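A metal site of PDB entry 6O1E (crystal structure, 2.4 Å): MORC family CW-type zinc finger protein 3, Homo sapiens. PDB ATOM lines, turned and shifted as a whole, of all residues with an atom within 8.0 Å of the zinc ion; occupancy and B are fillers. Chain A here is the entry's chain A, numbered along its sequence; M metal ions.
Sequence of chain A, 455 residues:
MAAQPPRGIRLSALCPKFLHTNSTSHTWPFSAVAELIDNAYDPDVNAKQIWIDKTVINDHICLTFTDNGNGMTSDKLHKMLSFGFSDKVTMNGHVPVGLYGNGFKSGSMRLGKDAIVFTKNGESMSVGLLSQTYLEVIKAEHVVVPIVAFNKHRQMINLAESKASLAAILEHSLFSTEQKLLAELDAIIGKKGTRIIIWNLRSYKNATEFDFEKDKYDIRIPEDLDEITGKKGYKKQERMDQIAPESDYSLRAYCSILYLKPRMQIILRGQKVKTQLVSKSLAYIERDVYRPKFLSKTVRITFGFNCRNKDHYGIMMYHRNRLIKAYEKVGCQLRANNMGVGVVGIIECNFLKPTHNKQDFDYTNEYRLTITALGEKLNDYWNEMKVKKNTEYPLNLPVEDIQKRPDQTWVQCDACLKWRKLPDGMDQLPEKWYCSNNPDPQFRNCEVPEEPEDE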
ATOM      1  N   GLN A 412     -15.709  -6.543  29.206  1.00  0.00           N
ATOM      2  CA  GLN A 412     -14.516  -6.355  30.002  1.00  0.00           C
ATOM      3  C   GLN A 412     -14.287  -7.543  30.941  1.00  0.00           C
ATOM      4  O   GLN A 412     -15.190  -7.944  31.689  1.00  0.00           O
ATOM      5  CB  GLN A 412     -14.641  -5.065  30.803  1.00  0.00           C
ATOM      6  CG  GLN A 412     -13.416  -4.671  31.542  1.00  0.00           C
ATOM      7  CD  GLN A 412     -13.583  -3.288  32.122  1.00  0.00           C
ATOM      8  OE1 GLN A 412     -14.657  -2.934  32.614  1.00  0.00           O
ATOM      9  NE2 GLN A 412     -12.525  -2.465  32.032  1.00  0.00           N
ATOM     10  N   CYS A 413     -13.086  -8.126  30.874  1.00  0.00           N
ATOM     11  CA  CYS A 413     -12.671  -9.092  31.883  1.00  0.00           C
ATOM     12  C   CYS A 413     -12.681  -8.454  33.258  1.00  0.00           C
ATOM     13  O   CYS A 413     -12.153  -7.356  33.449  1.00  0.00           O
ATOM     14  CB  CYS A 413     -11.267  -9.615  31.568  1.00  0.00           C
ATOM     15  SG  CYS A 413     -10.670 -10.860  32.775  1.00  0.00           S
ATOM     16  N   ASP A 414     -13.260  -9.157  34.229  1.00  0.00           N
ATOM     17  CA  ASP A 414     -13.321  -8.628  35.583  1.00  0.00           C
ATOM     18  C   ASP A 414     -12.035  -8.838  36.352  1.00  0.00           C
ATOM     19  O   ASP A 414     -11.829  -8.192  37.382  1.00  0.00           O
ATOM     20  CB  ASP A 414     -14.496  -9.234  36.339  1.00  0.00           C
ATOM     21  CG  ASP A 414     -15.782  -8.499  36.087  1.00  0.00           C
ATOM     22  OD1 ASP A 414     -16.067  -7.549  36.856  1.00  0.00           O
ATOM     23  OD2 ASP A 414     -16.494  -8.838  35.114  1.00  0.00           O
ATOM     24  N   ALA A 415     -11.142  -9.687  35.868  1.00  0.00           N
ATOM     25  CA  ALA A 415      -9.861  -9.871  36.532  1.00  0.00           C
ATOM     26  C   ALA A 415      -8.830  -8.867  36.007  1.00  0.00           C
ATOM     27  O   ALA A 415      -8.271  -8.100  36.800  1.00  0.00           O
ATOM     28  CB  ALA A 415      -9.361 -11.307  36.348  1.00  0.00           C
ATOM     29  N   CYS A 416      -8.593  -8.833  34.694  1.00  0.00           N
ATOM     30  CA  CYS A 416      -7.509  -8.021  34.133  1.00  0.00           C
ATOM     31  C   CYS A 416      -7.983  -6.724  33.478  1.00  0.00           C
ATOM     32  O   CYS A 416      -7.132  -5.966  33.009  1.00  0.00           O
ATOM     33  CB  CYS A 416      -6.732  -8.839  33.099  1.00  0.00           C
ATOM     34  SG  CYS A 416      -7.657  -9.167  31.536  1.00  0.00           S
ATOM     35  N   LEU A 417      -9.292  -6.480  33.389  1.00  0.00           N
ATOM     36  CA  LEU A 417      -9.898  -5.269  32.822  1.00  0.00           C
ATOM     37  C   LEU A 417      -9.642  -5.070  31.326  1.00  0.00           C
ATOM     38  O   LEU A 417      -9.996  -4.023  30.793  1.00  0.00           O
ATOM     39  CB  LEU A 417      -9.451  -4.010  33.578  1.00  0.00           C
ATOM     40  CG  LEU A 417      -9.657  -4.012  35.097  1.00  0.00           C
ATOM     41  CD1 LEU A 417      -9.539  -2.584  35.619  1.00  0.00           C
ATOM     42  CD2 LEU A 417     -10.993  -4.648  35.525  1.00  0.00           C
ATOM     43  N   LYS A 418      -9.082  -6.040  30.616  1.00  0.00           N
ATOM     44  CA  LYS A 418      -9.026  -5.939  29.166  1.00  0.00           C
ATOM     45  C   LYS A 418     -10.428  -6.092  28.550  1.00  0.00           C
ATOM     46  O   LYS A 418     -11.331  -6.693  29.143  1.00  0.00           O
ATOM     47  CB  LYS A 418      -8.102  -6.994  28.566  1.00  0.00           C
ATOM     48  CG  LYS A 418      -6.626  -6.828  28.905  1.00  0.00           C
ATOM     49  CD  LYS A 418      -5.784  -7.778  28.044  1.00  0.00           C
ATOM     50  CE  LYS A 418      -4.324  -7.774  28.495  1.00  0.00           C
ATOM     51  NZ  LYS A 418      -4.249  -8.200  29.915  1.00  0.00           N
ATOM     52  N   TRP A 419     -10.587  -5.536  27.360  1.00  0.00           N
ATOM     53  CA  TRP A 419     -11.843  -5.637  26.623  1.00  0.00           C
ATOM     54  C   TRP A 419     -11.734  -6.745  25.571  1.00  0.00           C
ATOM     55  O   TRP A 419     -10.720  -6.870  24.889  1.00  0.00           O
ATOM     56  CB  TRP A 419     -12.184  -4.306  25.965  1.00  0.00           C
ATOM     57  CG  TRP A 419     -12.708  -3.312  26.954  1.00  0.00           C
ATOM     58  CD1 TRP A 419     -11.991  -2.333  27.623  1.00  0.00           C
ATOM     59  CD2 TRP A 419     -14.068  -3.185  27.411  1.00  0.00           C
ATOM     60  NE1 TRP A 419     -12.836  -1.619  28.452  1.00  0.00           N
ATOM     61  CE2 TRP A 419     -14.110  -2.123  28.347  1.00  0.00           C
ATOM     62  CE3 TRP A 419     -15.258  -3.853  27.104  1.00  0.00           C
ATOM     63  CZ2 TRP A 419     -15.290  -1.728  28.969  1.00  0.00           C
ATOM     64  CZ3 TRP A 419     -16.427  -3.459  27.735  1.00  0.00           C
ATOM     65  CH2 TRP A 419     -16.437  -2.405  28.652  1.00  0.00           C
ATOM     66  N   ARG A 420     -12.781  -7.572  25.473  1.00  0.00           N
ATOM     67  CA  ARG A 420     -12.741  -8.707  24.551  1.00  0.00           C
ATOM     68  C   ARG A 420     -13.950  -8.673  23.636  1.00  0.00           C
ATOM     69  O   ARG A 420     -15.054  -8.312  24.052  1.00  0.00           O
ATOM     70  CB  ARG A 420     -12.715 -10.055  25.275  1.00  0.00           C
ATOM     71  CG  ARG A 420     -11.635 -10.169  26.309  1.00  0.00           C
ATOM     72  CD  ARG A 420     -10.291 -10.076  25.653  1.00  0.00           C
ATOM     73  NE  ARG A 420      -9.241 -10.594  26.516  1.00  0.00           N
ATOM     74  CZ  ARG A 420      -7.943 -10.507  26.253  1.00  0.00           C
ATOM     75  NH1 ARG A 420      -7.533  -9.932  25.123  1.00  0.00           N
ATOM     76  NH2 ARG A 420      -7.055 -11.014  27.094  1.00  0.00           N
ATOM     77  N   TRP A 433     -17.454 -11.665  34.356  1.00  0.00           N
ATOM     78  CA  TRP A 433     -16.994 -12.333  33.151  1.00  0.00           C
ATOM     79  C   TRP A 433     -15.480 -12.314  33.132  1.00  0.00           C
ATOM     80  O   TRP A 433     -14.871 -11.339  33.580  1.00  0.00           O
ATOM     81  CB  TRP A 433     -17.549 -11.648  31.899  1.00  0.00           C
ATOM     82  CG  TRP A 433     -17.289 -12.361  30.619  1.00  0.00           C
ATOM     83  CD1 TRP A 433     -18.130 -13.219  29.977  1.00  0.00           C
ATOM     84  CD2 TRP A 433     -16.117 -12.260  29.793  1.00  0.00           C
ATOM     85  NE1 TRP A 433     -17.549 -13.672  28.810  1.00  0.00           N
ATOM     86  CE2 TRP A 433     -16.306 -13.095  28.678  1.00  0.00           C
ATOM     87  CE3 TRP A 433     -14.909 -11.533  29.889  1.00  0.00           C
ATOM     88  CZ2 TRP A 433     -15.352 -13.228  27.658  1.00  0.00           C
ATOM     89  CZ3 TRP A 433     -13.959 -11.688  28.893  1.00  0.00           C
ATOM     90  CH2 TRP A 433     -14.185 -12.525  27.779  1.00  0.00           C
ATOM     91  N   TYR A 434     -14.878 -13.395  32.639  1.00  0.00           N
ATOM     92  CA  TYR A 434     -13.424 -13.516  32.664  1.00  0.00           C
ATOM     93  C   TYR A 434     -12.938 -14.041  31.331  1.00  0.00           C
ATOM     94  O   TYR A 434     -13.665 -14.769  30.644  1.00  0.00           O
ATOM     95  CB  TYR A 434     -12.936 -14.444  33.793  1.00  0.00           C
ATOM     96  CG  TYR A 434     -13.481 -14.058  35.135  1.00  0.00           C
ATOM     97  CD1 TYR A 434     -14.664 -14.610  35.608  1.00  0.00           C
ATOM     98  CD2 TYR A 434     -12.844 -13.105  35.924  1.00  0.00           C
ATOM     99  CE1 TYR A 434     -15.193 -14.240  36.847  1.00  0.00           C
ATOM    100  CE2 TYR A 434     -13.352 -12.722  37.161  1.00  0.00           C
ATOM    101  CZ  TYR A 434     -14.535 -13.293  37.610  1.00  0.00           C
ATOM    102  OH  TYR A 434     -15.059 -12.932  38.840  1.00  0.00           O
ATOM    103  N   CYS A 435     -11.706 -13.662  30.976  1.00  0.00           N
ATOM    104  CA  CYS A 435     -11.115 -14.104  29.718  1.00  0.00           C
ATOM    105  C   CYS A 435     -11.279 -15.608  29.532  1.00  0.00           C
ATOM    106  O   CYS A 435     -11.400 -16.095  28.392  1.00  0.00           O
ATOM    107  CB  CYS A 435      -9.629 -13.718  29.650  1.00  0.00           C
ATOM    108  SG  CYS A 435      -9.200 -11.919  29.540  1.00  0.00           S
ATOM    109  N   SER A 436     -11.281 -16.385  30.618  1.00  0.00           N
ATOM    110  CA  SER A 436     -11.409 -17.836  30.498  1.00  0.00           C
ATOM    111  C   SER A 436     -12.802 -18.257  30.027  1.00  0.00           C
ATOM    112  O   SER A 436     -12.950 -19.339  29.445  1.00  0.00           O
ATOM    113  CB  SER A 436     -11.066 -18.527  31.812  1.00  0.00           C
ATOM    114  OG  SER A 436     -11.879 -18.062  32.874  1.00  0.00           O
ATOM    115  N   PHE A 443      -8.279 -15.646  22.603  1.00  0.00           N
ATOM    116  CA  PHE A 443      -8.339 -14.592  23.607  1.00  0.00           C
ATOM    117  C   PHE A 443      -8.918 -15.127  24.902  1.00  0.00           C
ATOM    118  O   PHE A 443      -9.775 -14.489  25.540  1.00  0.00           O
ATOM    119  CB  PHE A 443      -9.151 -13.398  23.093  1.00  0.00           C
ATOM    120  CG  PHE A 443      -8.498 -12.698  21.936  1.00  0.00           C
ATOM    121  CD1 PHE A 443      -7.569 -11.686  22.155  1.00  0.00           C
ATOM    122  CD2 PHE A 443      -8.773 -13.095  20.638  1.00  0.00           C
ATOM    123  CE1 PHE A 443      -6.948 -11.049  21.075  1.00  0.00           C
ATOM    124  CE2 PHE A 443      -8.150 -12.456  19.545  1.00  0.00           C
ATOM    125  CZ  PHE A 443      -7.243 -11.422  19.772  1.00  0.00           C
ATOM    126  N   ARG A 444      -8.436 -16.293  25.336  1.00  0.00           N
ATOM    127  CA  ARG A 444      -8.998 -17.020  26.465  1.00  0.00           C
ATOM    128  C   ARG A 444      -8.107 -16.964  27.686  1.00  0.00           C
ATOM    129  O   ARG A 444      -8.356 -17.698  28.656  1.00  0.00           O
ATOM    130  CB  ARG A 444      -9.242 -18.470  26.066  1.00  0.00           C
ATOM    131  CG  ARG A 444     -10.430 -19.098  26.721  1.00  0.00           C
ATOM    132  CD  ARG A 444     -10.589 -20.495  26.221  1.00  0.00           C
ATOM    133  NE  ARG A 444     -11.322 -20.516  24.965  1.00  0.00           N
ATOM    134  CZ  ARG A 444     -11.529 -21.618  24.261  1.00  0.00           C
ATOM    135  NH1 ARG A 444     -11.040 -22.773  24.699  1.00  0.00           N
ATOM    136  NH2 ARG A 444     -12.215 -21.567  23.128  1.00  0.00           N
ATOM    137  N   ASN A 445      -7.096 -16.102  27.684  1.00  0.00           N
ATOM    138  CA  ASN A 445      -6.188 -15.952  28.816  1.00  0.00           C
ATOM    139  C   ASN A 445      -5.826 -14.476  28.975  1.00  0.00           C
ATOM    140  O   ASN A 445      -5.574 -13.774  27.984  1.00  0.00           O
ATOM    141  CB  ASN A 445      -4.930 -16.809  28.625  1.00  0.00           C
ATOM    142  CG  ASN A 445      -3.733 -16.279  29.386  1.00  0.00           C
ATOM    143  OD1 ASN A 445      -3.810 -15.956  30.581  1.00  0.00           O
ATOM    144  ND2 ASN A 445      -2.609 -16.155  28.682  1.00  0.00           N
ATOM    145  N   CYS A 446      -5.756 -14.025  30.231  1.00  0.00           N
ATOM    146  CA  CYS A 446      -5.536 -12.612  30.539  1.00  0.00           C
ATOM    147  C   CYS A 446      -4.207 -12.060  30.029  1.00  0.00           C
ATOM    148  O   CYS A 446      -4.010 -10.846  30.083  1.00  0.00           O
ATOM    149  CB  CYS A 446      -5.648 -12.422  32.059  1.00  0.00           C
ATOM    150  SG  CYS A 446      -7.328 -12.847  32.702  1.00  0.00           S
ATOM    151  N   GLU A 447      -3.296 -12.900  29.534  1.00  0.00           N
ATOM    152  CA  GLU A 447      -2.009 -12.408  29.057  1.00  0.00           C
ATOM    153  C   GLU A 447      -2.054 -11.940  27.605  1.00  0.00           C
ATOM    154  O   GLU A 447      -1.142 -11.216  27.168  1.00  0.00           O
ATOM    155  CB  GLU A 447      -0.933 -13.490  29.181  1.00  0.00           C
ATOM    156  CG  GLU A 447      -0.797 -14.094  30.554  1.00  0.00           C
ATOM    157  CD  GLU A 447       0.213 -13.357  31.401  1.00  0.00           C
ATOM    158  OE1 GLU A 447       1.056 -14.022  32.044  1.00  0.00           O
ATOM    159  OE2 GLU A 447       0.170 -12.105  31.398  1.00  0.00           O
ATOM    160  N   VAL A 448      -3.038 -12.370  26.851  1.00  0.00           N
ATOM    161  CA  VAL A 448      -3.105 -11.986  25.438  1.00  0.00           C
ATOM    162  C   VAL A 448      -3.441 -10.510  25.348  1.00  0.00           C
ATOM    163  O   VAL A 448      -4.412 -10.056  25.977  1.00  0.00           O
ATOM    164  CB  VAL A 448      -4.148 -12.841  24.709  1.00  0.00           C
ATOM    165  CG1 VAL A 448      -4.123 -12.553  23.233  1.00  0.00           C
ATOM    166  CG2 VAL A 448      -3.909 -14.330  24.978  1.00  0.00           C
HETATM  167 ZN    ZN M   1      -8.724 -11.224  31.719  1.00  0.00          ZN
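The backbone NH (N) of Cys 413 lies within hydrogen-bond range of the backbone carbonyl oxygen (O) of Lys 418 (2.9 Å). The side-chain sulfur (SG) of Cys 413 sits close to the backbone NH (N) of Ala 415 (3.3 Å). O of Cys 446 sits at hydrogen-bond distance from NZ of Lys 418 (2.7 Å). The guanidinium group (NE) of Arg 420 sits close to the side-chain sulfur (SG) of Cys 435, 3.3 Å away. The backbone NH (N) of Lys 418 lies close to the side-chain sulfur (SG) of Cys 416, at 3.6 Å.
Four residues have an atom within 4 Å of the zinc ion: Cys 413, Cys 416, Cys 435 and Cys 446. Along chain A the residues within 4 Å of the zinc ion span positions 413 to 446.
The zinc ion is bound by SG of Cys 413, at 2.2 Å. SG of Cys 416 is bound to the zinc ion (2.3 Å). SG of Cys 435 is bound to the zinc ion, at 2.3 Å. The zinc ion is bound by SG of Cys 446. The zinc ion has four donor atoms within binding distance.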
